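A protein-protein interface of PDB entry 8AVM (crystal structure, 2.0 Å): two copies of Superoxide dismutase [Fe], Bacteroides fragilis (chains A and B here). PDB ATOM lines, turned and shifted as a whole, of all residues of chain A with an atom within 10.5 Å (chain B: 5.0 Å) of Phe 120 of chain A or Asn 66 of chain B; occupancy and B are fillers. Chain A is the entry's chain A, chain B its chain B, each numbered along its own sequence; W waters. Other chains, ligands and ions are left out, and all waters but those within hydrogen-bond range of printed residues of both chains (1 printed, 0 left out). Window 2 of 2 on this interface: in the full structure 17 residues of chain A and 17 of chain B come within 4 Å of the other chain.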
ATOM      1  N   ASN A 113     -11.164  13.395  22.248  1.00  0.00           N
ATOM      2  CA  ASN A 113     -12.070  14.251  21.508  1.00  0.00           C
ATOM      3  C   ASN A 113     -11.335  14.978  20.397  1.00  0.00           C
ATOM      4  O   ASN A 113     -11.849  15.049  19.294  1.00  0.00           O
ATOM      5  CB  ASN A 113     -12.757  15.279  22.409  1.00  0.00           C
ATOM      6  CG  ASN A 113     -13.831  14.625  23.274  1.00  0.00           C
ATOM      7  OD1 ASN A 113     -14.249  13.502  23.015  1.00  0.00           O
ATOM      8  ND2 ASN A 113     -14.330  15.328  24.272  1.00  0.00           N
ATOM      9  N   ALA A 114     -10.162  15.533  20.706  1.00  0.00           N
ATOM     10  CA  ALA A 114      -9.414  16.304  19.720  1.00  0.00           C
ATOM     11  C   ALA A 114      -8.948  15.387  18.588  1.00  0.00           C
ATOM     12  O   ALA A 114      -9.005  15.767  17.426  1.00  0.00           O
ATOM     13  CB  ALA A 114      -8.234  17.030  20.350  1.00  0.00           C
ATOM     14  N   ALA A 115      -8.498  14.188  18.916  1.00  0.00           N
ATOM     15  CA  ALA A 115      -8.123  13.245  17.865  1.00  0.00           C
ATOM     16  C   ALA A 115      -9.340  12.879  17.004  1.00  0.00           C
ATOM     17  O   ALA A 115      -9.256  12.793  15.792  1.00  0.00           O
ATOM     18  CB  ALA A 115      -7.491  12.016  18.469  1.00  0.00           C
ATOM     19  N   SER A 116     -10.484  12.687  17.647  1.00  0.00           N
ATOM     20  CA  SER A 116     -11.699  12.305  16.941  1.00  0.00           C
ATOM     21  C   SER A 116     -12.142  13.421  15.995  1.00  0.00           C
ATOM     22  O   SER A 116     -12.427  13.180  14.819  1.00  0.00           O
ATOM     23  CB  SER A 116     -12.811  11.950  17.934  1.00  0.00           C
ATOM     24  OG  SER A 116     -12.413  10.840  18.741  1.00  0.00           O
ATOM     25  N   VAL A 117     -12.176  14.655  16.524  1.00  0.00           N
ATOM     26  CA  VAL A 117     -12.706  15.764  15.745  1.00  0.00           C
ATOM     27  C   VAL A 117     -11.681  16.151  14.678  1.00  0.00           C
ATOM     28  O   VAL A 117     -12.062  16.614  13.624  1.00  0.00           O
ATOM     29  CB  VAL A 117     -13.057  16.944  16.664  1.00  0.00           C
ATOM     30  CG1 VAL A 117     -13.316  18.235  15.881  1.00  0.00           C
ATOM     31  CG2 VAL A 117     -14.255  16.571  17.544  1.00  0.00           C
ATOM     32  N   GLY A 118     -10.387  15.961  14.957  1.00  0.00           N
ATOM     33  CA  GLY A 118      -9.340  16.453  14.076  1.00  0.00           C
ATOM     34  C   GLY A 118      -8.981  15.477  12.965  1.00  0.00           C
ATOM     35  O   GLY A 118      -8.187  15.788  12.096  1.00  0.00           O
ATOM     36  N   LEU A 119      -9.541  14.278  12.949  1.00  0.00           N
ATOM     37  CA  LEU A 119      -9.179  13.329  11.904  1.00  0.00           C
ATOM     38  C   LEU A 119      -9.902  13.732  10.618  1.00  0.00           C
ATOM     39  O   LEU A 119     -11.135  13.707  10.563  1.00  0.00           O
ATOM     40  CB  LEU A 119      -9.545  11.912  12.357  1.00  0.00           C
ATOM     41  CG  LEU A 119      -8.929  10.747  11.573  1.00  0.00           C
ATOM     42  CD1 LEU A 119      -9.096   9.447  12.361  1.00  0.00           C
ATOM     43  CD2 LEU A 119      -9.573  10.568  10.183  1.00  0.00           C
ATOM     44  N   PHE A 120      -9.128  14.090   9.581  1.00  0.00           N
ATOM     45  CA  PHE A 120      -9.720  14.599   8.344  1.00  0.00           C
ATOM     46  C   PHE A 120     -10.119  13.445   7.441  1.00  0.00           C
ATOM     47  O   PHE A 120      -9.316  12.532   7.222  1.00  0.00           O
ATOM     48  CB  PHE A 120      -8.726  15.489   7.609  1.00  0.00           C
ATOM     49  CG  PHE A 120      -9.381  16.283   6.502  1.00  0.00           C
ATOM     50  CD1 PHE A 120     -10.271  17.308   6.800  1.00  0.00           C
ATOM     51  CD2 PHE A 120      -9.133  15.972   5.174  1.00  0.00           C
ATOM     52  CE1 PHE A 120     -10.857  18.044   5.791  1.00  0.00           C
ATOM     53  CE2 PHE A 120      -9.743  16.684   4.158  1.00  0.00           C
ATOM     54  CZ  PHE A 120     -10.611  17.710   4.461  1.00  0.00           C
ATOM     55  N   GLY A 121     -11.366  13.431   6.948  1.00  0.00           N
ATOM     56  CA  GLY A 121     -11.817  12.302   6.141  1.00  0.00           C
ATOM     57  C   GLY A 121     -12.370  11.167   7.028  1.00  0.00           C
ATOM     58  O   GLY A 121     -12.966  11.411   8.076  1.00  0.00           O
ATOM     59  N   SER A 122     -12.250   9.935   6.512  1.00  0.00           N
ATOM     60  CA  SER A 122     -12.762   8.723   7.119  1.00  0.00           C
ATOM     61  C   SER A 122     -11.660   8.097   7.972  1.00  0.00           C
ATOM     62  O   SER A 122     -10.494   8.079   7.600  1.00  0.00           O
ATOM     63  CB  SER A 122     -13.257   7.751   6.069  1.00  0.00           C
ATOM     64  OG  SER A 122     -14.303   8.351   5.257  1.00  0.00           O
ATOM     65  N   GLY A 123     -12.040   7.574   9.122  1.00  0.00           N
ATOM     66  CA  GLY A 123     -11.109   6.865   9.972  1.00  0.00           C
ATOM     67  C   GLY A 123     -11.677   6.598  11.370  1.00  0.00           C
ATOM     68  O   GLY A 123     -12.880   6.687  11.589  1.00  0.00           O
ATOM     69  N   TRP A 124     -10.774   6.249  12.278  1.00  0.00           N
ATOM     70  CA  TRP A 124     -11.045   5.847  13.641  1.00  0.00           C
ATOM     71  C   TRP A 124     -10.054   6.520  14.592  1.00  0.00           C
ATOM     72  O   TRP A 124      -8.847   6.461  14.384  1.00  0.00           O
ATOM     73  CB  TRP A 124     -10.889   4.325  13.759  1.00  0.00           C
ATOM     74  CG  TRP A 124     -11.752   3.578  12.812  1.00  0.00           C
ATOM     75  CD1 TRP A 124     -11.601   3.419  11.463  1.00  0.00           C
ATOM     76  CD2 TRP A 124     -12.990   2.959  13.153  1.00  0.00           C
ATOM     77  NE1 TRP A 124     -12.657   2.735  10.936  1.00  0.00           N
ATOM     78  CE2 TRP A 124     -13.529   2.439  11.953  1.00  0.00           C
ATOM     79  CE3 TRP A 124     -13.684   2.797  14.356  1.00  0.00           C
ATOM     80  CZ2 TRP A 124     -14.732   1.754  11.937  1.00  0.00           C
ATOM     81  CZ3 TRP A 124     -14.871   2.105  14.331  1.00  0.00           C
ATOM     82  CH2 TRP A 124     -15.380   1.599  13.138  1.00  0.00           C
ATOM     83  N   ALA A 125     -10.558   7.173  15.639  1.00  0.00           N
ATOM     84  CA  ALA A 125      -9.711   7.512  16.777  1.00  0.00           C
ATOM     85  C   ALA A 125      -9.658   6.325  17.732  1.00  0.00           C
ATOM     86  O   ALA A 125     -10.707   5.748  18.059  1.00  0.00           O
ATOM     87  CB  ALA A 125     -10.266   8.737  17.476  1.00  0.00           C
ATOM     88  N   THR A 138      -4.233   7.061  18.742  1.00  0.00           N
ATOM     89  CA  THR A 138      -3.853   7.195  17.341  1.00  0.00           C
ATOM     90  C   THR A 138      -5.086   7.570  16.516  1.00  0.00           C
ATOM     91  O   THR A 138      -6.232   7.312  16.892  1.00  0.00           O
ATOM     92  CB  THR A 138      -3.232   5.901  16.805  1.00  0.00           C
ATOM     93  OG1 THR A 138      -4.192   4.849  16.972  1.00  0.00           O
ATOM     94  CG2 THR A 138      -1.938   5.540  17.519  1.00  0.00           C
ATOM     95  N   LYS A 139      -4.817   8.169  15.369  1.00  0.00           N
ATOM     96  CA  LYS A 139      -5.785   8.380  14.308  1.00  0.00           C
ATOM     97  C   LYS A 139      -5.530   7.353  13.224  1.00  0.00           C
ATOM     98  O   LYS A 139      -4.487   7.397  12.623  1.00  0.00           O
ATOM     99  CB  LYS A 139      -5.629   9.798  13.774  1.00  0.00           C
ATOM    100  CG  LYS A 139      -5.951  10.841  14.830  1.00  0.00           C
ATOM    101  CD  LYS A 139      -6.169  12.248  14.336  1.00  0.00           C
ATOM    102  CE  LYS A 139      -4.927  13.096  14.308  1.00  0.00           C
ATOM    103  NZ  LYS A 139      -5.256  14.277  13.498  1.00  0.00           N
ATOM    104  N   GLU A 140      -6.457   6.419  13.033  1.00  0.00           N
ATOM    105  CA  GLU A 140      -6.305   5.395  12.026  1.00  0.00           C
ATOM    106  C   GLU A 140      -7.117   5.802  10.808  1.00  0.00           C
ATOM    107  O   GLU A 140      -8.333   5.909  10.906  1.00  0.00           O
ATOM    108  CB  GLU A 140      -6.772   4.058  12.584  1.00  0.00           C
ATOM    109  CG  GLU A 140      -6.011   3.651  13.851  1.00  0.00           C
ATOM    110  CD  GLU A 140      -4.531   3.351  13.652  1.00  0.00           C
ATOM    111  OE1 GLU A 140      -3.740   3.513  14.627  1.00  0.00           O
ATOM    112  OE2 GLU A 140      -4.190   2.934  12.557  1.00  0.00           O
ATOM    113  N   PRO A 141      -6.491   6.044   9.637  1.00  0.00           N
ATOM    114  CA  PRO A 141      -7.235   6.410   8.442  1.00  0.00           C
ATOM    115  C   PRO A 141      -8.022   5.230   7.902  1.00  0.00           C
ATOM    116  O   PRO A 141      -7.606   4.076   7.970  1.00  0.00           O
ATOM    117  CB  PRO A 141      -6.163   6.890   7.429  1.00  0.00           C
ATOM    118  CG  PRO A 141      -4.885   6.213   7.890  1.00  0.00           C
ATOM    119  CD  PRO A 141      -5.033   5.993   9.393  1.00  0.00           C
ATOM    120  N   ASN A 142      -9.215   5.544   7.392  1.00  0.00           N
ATOM    121  CA  ASN A 142     -10.003   4.597   6.610  1.00  0.00           C
ATOM    122  C   ASN A 142     -10.272   3.343   7.435  1.00  0.00           C
ATOM    123  O   ASN A 142     -10.963   3.406   8.461  1.00  0.00           O
ATOM    124  CB  ASN A 142      -9.340   4.388   5.238  1.00  0.00           C
ATOM    125  CG  ASN A 142      -9.371   5.663   4.410  1.00  0.00           C
ATOM    126  OD1 ASN A 142     -10.197   6.545   4.630  1.00  0.00           O
ATOM    127  ND2 ASN A 142      -8.434   5.807   3.494  1.00  0.00           N
ATOM    128  N   GLY A 143      -9.764   2.190   6.965  1.00  0.00           N
ATOM    129  CA  GLY A 143     -10.066   0.900   7.569  1.00  0.00           C
ATOM    130  C   GLY A 143      -9.001   0.406   8.542  1.00  0.00           C
ATOM    131  O   GLY A 143      -9.076  -0.720   9.058  1.00  0.00           O
ATOM    132  N   VAL A 159     -15.233   7.793  12.917  1.00  0.00           N
ATOM    133  CA  VAL A 159     -15.550   9.119  12.407  1.00  0.00           C
ATOM    134  C   VAL A 159     -15.806   9.108  10.902  1.00  0.00           C
ATOM    135  O   VAL A 159     -15.919  10.180  10.310  1.00  0.00           O
ATOM    136  CB  VAL A 159     -14.515  10.189  12.806  1.00  0.00           C
ATOM    137  CG1 VAL A 159     -14.444  10.365  14.300  1.00  0.00           C
ATOM    138  CG2 VAL A 159     -13.146   9.926  12.215  1.00  0.00           C
ATOM    139  N   TRP A 160     -15.964   7.920  10.301  1.00  0.00           N
ATOM    140  CA  TRP A 160     -16.640   7.823   9.033  1.00  0.00           C
ATOM    141  C   TRP A 160     -17.983   8.531   9.189  1.00  0.00           C
ATOM    142  O   TRP A 160     -18.687   8.356  10.183  1.00  0.00           O
ATOM    143  CB  TRP A 160     -16.872   6.368   8.613  1.00  0.00           C
ATOM    144  CG  TRP A 160     -15.661   5.608   8.175  1.00  0.00           C
ATOM    145  CD1 TRP A 160     -14.548   5.332   8.910  1.00  0.00           C
ATOM    146  CD2 TRP A 160     -15.461   5.010   6.894  1.00  0.00           C
ATOM    147  NE1 TRP A 160     -13.677   4.592   8.174  1.00  0.00           N
ATOM    148  CE2 TRP A 160     -14.204   4.370   6.935  1.00  0.00           C
ATOM    149  CE3 TRP A 160     -16.224   4.925   5.718  1.00  0.00           C
ATOM    150  CZ2 TRP A 160     -13.674   3.705   5.822  1.00  0.00           C
ATOM    151  CZ3 TRP A 160     -15.734   4.210   4.642  1.00  0.00           C
ATOM    152  CH2 TRP A 160     -14.464   3.626   4.687  1.00  0.00           C
ATOM    153  N   GLU A 161     -18.367   9.280   8.177  1.00  0.00           N
ATOM    154  CA  GLU A 161     -19.602  10.072   8.309  1.00  0.00           C
ATOM    155  C   GLU A 161     -20.848   9.197   8.532  1.00  0.00           C
ATOM    156  O   GLU A 161     -21.787   9.608   9.218  1.00  0.00           O
ATOM    157  CB  GLU A 161     -19.744  10.987   7.095  1.00  0.00           C
ATOM    158  CG  GLU A 161     -18.752  12.165   7.171  1.00  0.00           C
ATOM    159  CD  GLU A 161     -18.725  13.079   5.957  1.00  0.00           C
ATOM    160  OE1 GLU A 161     -18.787  12.578   4.804  1.00  0.00           O
ATOM    161  OE2 GLU A 161     -18.745  14.287   6.166  1.00  0.00           O
ATOM    162  N   TYR A 164     -22.474   8.893  12.015  1.00  0.00           N
ATOM    163  CA  TYR A 164     -23.178   9.979  12.682  1.00  0.00           C
ATOM    164  C   TYR A 164     -24.079  10.813  11.769  1.00  0.00           C
ATOM    165  O   TYR A 164     -24.879  11.614  12.254  1.00  0.00           O
ATOM    166  CB  TYR A 164     -22.183  10.892  13.399  1.00  0.00           C
ATOM    167  CG  TYR A 164     -21.126  11.567  12.571  1.00  0.00           C
ATOM    168  CD1 TYR A 164     -21.368  12.740  11.856  1.00  0.00           C
ATOM    169  CD2 TYR A 164     -19.847  11.031  12.492  1.00  0.00           C
ATOM    170  CE1 TYR A 164     -20.367  13.370  11.120  1.00  0.00           C
ATOM    171  CE2 TYR A 164     -18.851  11.638  11.730  1.00  0.00           C
ATOM    172  CZ  TYR A 164     -19.094  12.804  11.048  1.00  0.00           C
ATOM    173  OH  TYR A 164     -18.042  13.430  10.345  1.00  0.00           O
ATOM    174  N   ARG A 172     -19.971  16.634  13.775  1.00  0.00           N
ATOM    175  CA  ARG A 172     -19.188  15.522  14.313  1.00  0.00           C
ATOM    176  C   ARG A 172     -18.877  15.706  15.791  1.00  0.00           C
ATOM    177  O   ARG A 172     -18.970  14.730  16.579  1.00  0.00           O
ATOM    178  CB  ARG A 172     -17.904  15.323  13.521  1.00  0.00           C
ATOM    179  CG  ARG A 172     -17.119  14.095  13.963  1.00  0.00           C
ATOM    180  CD  ARG A 172     -15.681  14.003  13.475  1.00  0.00           C
ATOM    181  NE  ARG A 172     -15.603  13.728  12.061  1.00  0.00           N
ATOM    182  CZ  ARG A 172     -14.441  13.630  11.411  1.00  0.00           C
ATOM    183  NH1 ARG A 172     -14.410  13.361  10.111  1.00  0.00           N
ATOM    184  NH2 ARG A 172     -13.320  13.700  12.119  1.00  0.00           N
ATOM    185  N   TYR B  34     -15.607  24.884   5.080  1.00  0.00           N
ATOM    186  CA  TYR B  34     -14.301  24.849   4.430  1.00  0.00           C
ATOM    187  C   TYR B  34     -13.836  26.259   4.073  1.00  0.00           C
ATOM    188  O   TYR B  34     -12.671  26.586   4.265  1.00  0.00           O
ATOM    189  CB  TYR B  34     -14.309  23.962   3.181  1.00  0.00           C
ATOM    190  CG  TYR B  34     -14.556  22.497   3.460  1.00  0.00           C
ATOM    191  CD1 TYR B  34     -13.815  21.796   4.398  1.00  0.00           C
ATOM    192  CD2 TYR B  34     -15.505  21.801   2.746  1.00  0.00           C
ATOM    193  CE1 TYR B  34     -13.989  20.444   4.593  1.00  0.00           C
ATOM    194  CE2 TYR B  34     -15.720  20.446   2.955  1.00  0.00           C
ATOM    195  CZ  TYR B  34     -14.955  19.768   3.875  1.00  0.00           C
ATOM    196  OH  TYR B  34     -15.179  18.431   4.040  1.00  0.00           O
ATOM    197  N   GLY B  62      -1.763  18.970   4.978  1.00  0.00           N
ATOM    198  CA  GLY B  62      -2.032  19.809   6.128  1.00  0.00           C
ATOM    199  C   GLY B  62      -3.400  20.438   5.997  1.00  0.00           C
ATOM    200  O   GLY B  62      -4.105  20.166   5.010  1.00  0.00           O
ATOM    201  N   ALA B  63      -3.737  21.284   6.982  1.00  0.00           N
ATOM    202  CA  ALA B  63      -5.086  21.796   7.132  1.00  0.00           C
ATOM    203  C   ALA B  63      -5.390  22.780   6.005  1.00  0.00           C
ATOM    204  O   ALA B  63      -6.501  22.835   5.483  1.00  0.00           O
ATOM    205  CB  ALA B  63      -5.297  22.419   8.512  1.00  0.00           C
ATOM    206  N   ILE B  64      -4.398  23.584   5.635  1.00  0.00           N
ATOM    207  CA  ILE B  64      -4.592  24.546   4.571  1.00  0.00           C
ATOM    208  C   ILE B  64      -4.890  23.807   3.272  1.00  0.00           C
ATOM    209  O   ILE B  64      -5.861  24.138   2.596  1.00  0.00           O
ATOM    210  CB  ILE B  64      -3.379  25.490   4.507  1.00  0.00           C
ATOM    211  CG1 ILE B  64      -3.535  26.553   5.609  1.00  0.00           C
ATOM    212  CG2 ILE B  64      -3.243  26.139   3.151  1.00  0.00           C
ATOM    213  CD1 ILE B  64      -2.315  27.320   5.975  1.00  0.00           C
ATOM    214  N   PHE B  65      -4.074  22.800   2.948  1.00  0.00           N
ATOM    215  CA  PHE B  65      -4.317  22.033   1.744  1.00  0.00           C
ATOM    216  C   PHE B  65      -5.705  21.377   1.791  1.00  0.00           C
ATOM    217  O   PHE B  65      -6.458  21.430   0.831  1.00  0.00           O
ATOM    218  CB  PHE B  65      -3.248  20.961   1.575  1.00  0.00           C
ATOM    219  CG  PHE B  65      -3.494  20.127   0.348  1.00  0.00           C
ATOM    220  CD1 PHE B  65      -3.194  20.601  -0.912  1.00  0.00           C
ATOM    221  CD2 PHE B  65      -4.081  18.865   0.465  1.00  0.00           C
ATOM    222  CE1 PHE B  65      -3.424  19.817  -2.041  1.00  0.00           C
ATOM    223  CE2 PHE B  65      -4.316  18.095  -0.657  1.00  0.00           C
ATOM    224  CZ  PHE B  65      -3.991  18.568  -1.911  1.00  0.00           C
ATOM    225  N   ASN B  66      -6.028  20.763   2.936  1.00  0.00           N
ATOM    226  CA  ASN B  66      -7.285  20.061   3.099  1.00  0.00           C
ATOM    227  C   ASN B  66      -8.450  20.998   2.779  1.00  0.00           C
ATOM    228  O   ASN B  66      -9.379  20.632   2.069  1.00  0.00           O
ATOM    229  CB  ASN B  66      -7.429  19.519   4.512  1.00  0.00           C
ATOM    230  CG  ASN B  66      -6.606  18.282   4.791  1.00  0.00           C
ATOM    231  OD1 ASN B  66      -6.081  17.658   3.866  1.00  0.00           O
ATOM    232  ND2 ASN B  66      -6.574  17.896   6.067  1.00  0.00           N
ATOM    233  N   ASN B  67      -8.396  22.220   3.311  1.00  0.00           N
ATOM    234  CA  ASN B  67      -9.519  23.127   3.202  1.00  0.00           C
ATOM    235  C   ASN B  67      -9.552  23.730   1.810  1.00  0.00           C
ATOM    236  O   ASN B  67     -10.630  23.837   1.222  1.00  0.00           O
ATOM    237  CB  ASN B  67      -9.524  24.153   4.334  1.00  0.00           C
ATOM    238  CG  ASN B  67      -9.971  23.523   5.636  1.00  0.00           C
ATOM    239  OD1 ASN B  67     -11.150  23.308   5.808  1.00  0.00           O
ATOM    240  ND2 ASN B  67      -9.049  23.159   6.517  1.00  0.00           N
ATOM    241  N   ALA B  68      -8.383  24.136   1.283  1.00  0.00           N
ATOM    242  CA  ALA B  68      -8.348  24.704  -0.050  1.00  0.00           C
ATOM    243  C   ALA B  68      -8.823  23.687  -1.071  1.00  0.00           C
ATOM    244  O   ALA B  68      -9.609  23.993  -1.984  1.00  0.00           O
ATOM    245  CB  ALA B  68      -6.926  25.120  -0.382  1.00  0.00           C
ATOM    246  N   GLY B  69      -8.293  22.463  -0.954  1.00  0.00           N
ATOM    247  CA  GLY B  69      -8.717  21.410  -1.858  1.00  0.00           C
ATOM    248  C   GLY B  69     -10.229  21.212  -1.824  1.00  0.00           C
ATOM    249  O   GLY B  69     -10.845  21.035  -2.847  1.00  0.00           O
ATOM    250  N   GLN B  70     -10.824  21.248  -0.641  1.00  0.00           N
ATOM    251  CA  GLN B  70     -12.241  21.013  -0.490  1.00  0.00           C
ATOM    252  C   GLN B  70     -13.012  22.192  -1.053  1.00  0.00           C
ATOM    253  O   GLN B  70     -14.076  21.985  -1.662  1.00  0.00           O
ATOM    254  CB  GLN B  70     -12.610  20.699   0.969  1.00  0.00           C
ATOM    255  CG  GLN B  70     -12.259  19.281   1.384  1.00  0.00           C
ATOM    256  CD  GLN B  70     -12.994  18.206   0.619  1.00  0.00           C
ATOM    257  OE1 GLN B  70     -12.639  17.903  -0.517  1.00  0.00           O
ATOM    258  NE2 GLN B  70     -14.008  17.615   1.246  1.00  0.00           N
ATOM    259  N   ASN B 142      -9.640  12.213   0.191  1.00  0.00           N
ATOM    260  CA  ASN B 142      -9.928  13.273   1.146  1.00  0.00           C
ATOM    261  C   ASN B 142     -10.149  14.583   0.403  1.00  0.00           C
ATOM    262  O   ASN B 142     -11.116  14.702  -0.365  1.00  0.00           O
ATOM    263  CB  ASN B 142      -8.905  13.301   2.275  1.00  0.00           C
ATOM    264  CG  ASN B 142      -8.911  12.024   3.086  1.00  0.00           C
ATOM    265  OD1 ASN B 142      -9.909  11.299   3.127  1.00  0.00           O
ATOM    266  ND2 ASN B 142      -7.793  11.752   3.743  1.00  0.00           N
ATOM    267  N   GLY B 143      -9.290  15.591   0.645  1.00  0.00           N
ATOM    268  CA  GLY B 143      -9.509  16.919   0.080  1.00  0.00           C
ATOM    269  C   GLY B 143      -8.676  17.194  -1.155  1.00  0.00           C
ATOM    270  O   GLY B 143      -8.699  18.292  -1.692  1.00  0.00           O
ATOM    271  N   TRP B 160     -17.273  11.425  -0.606  1.00  0.00           N
ATOM    272  CA  TRP B 160     -17.523  11.607   0.809  1.00  0.00           C
ATOM    273  C   TRP B 160     -18.964  11.206   1.065  1.00  0.00           C
ATOM    274  O   TRP B 160     -19.863  11.601   0.331  1.00  0.00           O
ATOM    275  CB  TRP B 160     -17.301  13.059   1.262  1.00  0.00           C
ATOM    276  CG  TRP B 160     -15.872  13.504   1.306  1.00  0.00           C
ATOM    277  CD1 TRP B 160     -14.995  13.602   0.265  1.00  0.00           C
ATOM    278  CD2 TRP B 160     -15.181  13.986   2.467  1.00  0.00           C
ATOM    279  NE1 TRP B 160     -13.795  14.087   0.704  1.00  0.00           N
ATOM    280  CE2 TRP B 160     -13.884  14.361   2.044  1.00  0.00           C
ATOM    281  CE3 TRP B 160     -15.534  14.183   3.808  1.00  0.00           C
ATOM    282  CZ2 TRP B 160     -12.925  14.848   2.940  1.00  0.00           C
ATOM    283  CZ3 TRP B 160     -14.604  14.688   4.687  1.00  0.00           C
ATOM    284  CH2 TRP B 160     -13.313  15.045   4.249  1.00  0.00           C
HETATM  285  O   HOH W   1     -11.016   8.995   3.947  1.00  0.00           O
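Water W1 lies within hydrogen-bond range of OD1 of Asn 142 of chain A (2.7 Å), OD1 of Asn 142 of chain B (2.7 Å) and N of Ser 122 of chain A (3.0 Å).
Of chain B, only Asn 66, Gln 70, Asn 142, Gly 143 and Trp 160 come within 4 Å of Phe 120 of chain A. Asn 66 of chain B touches just one residue of chain A: Phe 120 (3.3 Å). No residue of chain A comes within 4 Å of Gly 62 of chain B. No residue of chain A comes within 4 Å of Ala 63 of chain B. No residue of chain A comes within 4 Å of Asn 67 of chain B. No residue of chain A comes within 4 Å of Ala 68 of chain B. No residue of chain A comes within 4 Å of Gly 69 of chain B. Of chain A, only Phe 120 (3.8 Å) comes within 4 Å of Gln 70 of chain B. Gly 143 of chain B touches just one residue of chain A: Phe 120. Of the printed residues of chain B, Glu 161 of chain A touches Trp 160. Printed residues of chain B within 4 Å of Gly 121 of chain A: Asn 142 and Trp 160. The nearest printed residue of chain A that does not touch Asn 66 of chain B is Gly 118 of chain A (6.6 Å). The nearest printed residue of chain A that does not touch Trp 160 of chain B is Arg 172 of chain A (5.6 Å).
Hydrophobic or aromatic side chains of chain B that line the printed part of chain A: Trp 160. Hydrophobic or aromatic side chains of chain A within 4 Å of the printed part of chain B: Phe 120. Among the printed residues, no Asp or Glu carboxylate lies within 4 Å of a Lys or Arg side-chain nitrogen of the other chain.
NH1 of Arg 172 of chain A is in hydrogen-bond range of O of Gly 121 of chain A. The side-chain hydroxyl (OH) of Tyr 34 of chain B lies within hydrogen-bond range of the side-chain amide nitrogen (NE2) of Gln 70 of chain B, 3.1 Å away. NE1 of Trp 160 of chain B sits at hydrogen-bond distance from O of Asn 142 of chain B (2.9 Å). The side-chain amide oxygen of Asn 66 of chain B lies close to the backbone carbonyl oxygen of Gly 62 of chain B, 3.4 Å away.
Phe 120 of chain A touches Asn 66 of chain B. Phe 120 of chain A touches Gln 70 of chain B. Asn 142 of chain B touches Phe 120 of chain A. Gly 143 of chain B touches Phe 120 of chain A (N to CE2, 3.7 Å). CH2 of Trp 160 of chain B touches CZ of Phe 120 of chain A, 3.8 Å away. Asn 142 of chain B touches Gly 121 of chain A (OD1 to CA, 3.7 Å). Trp 160 of chain B touches Gly 121 of chain A (CH2 to CA, 3.7 Å). OE1 of Glu 161 of chain A touches CE3 of Trp 160 of chain B (3.8 Å).
Positions printed for both chains: 142, 143 and 160. Of the 8 pairs that touch across the chains among the printed residues, none has its exchanged pair printed and touching as well.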
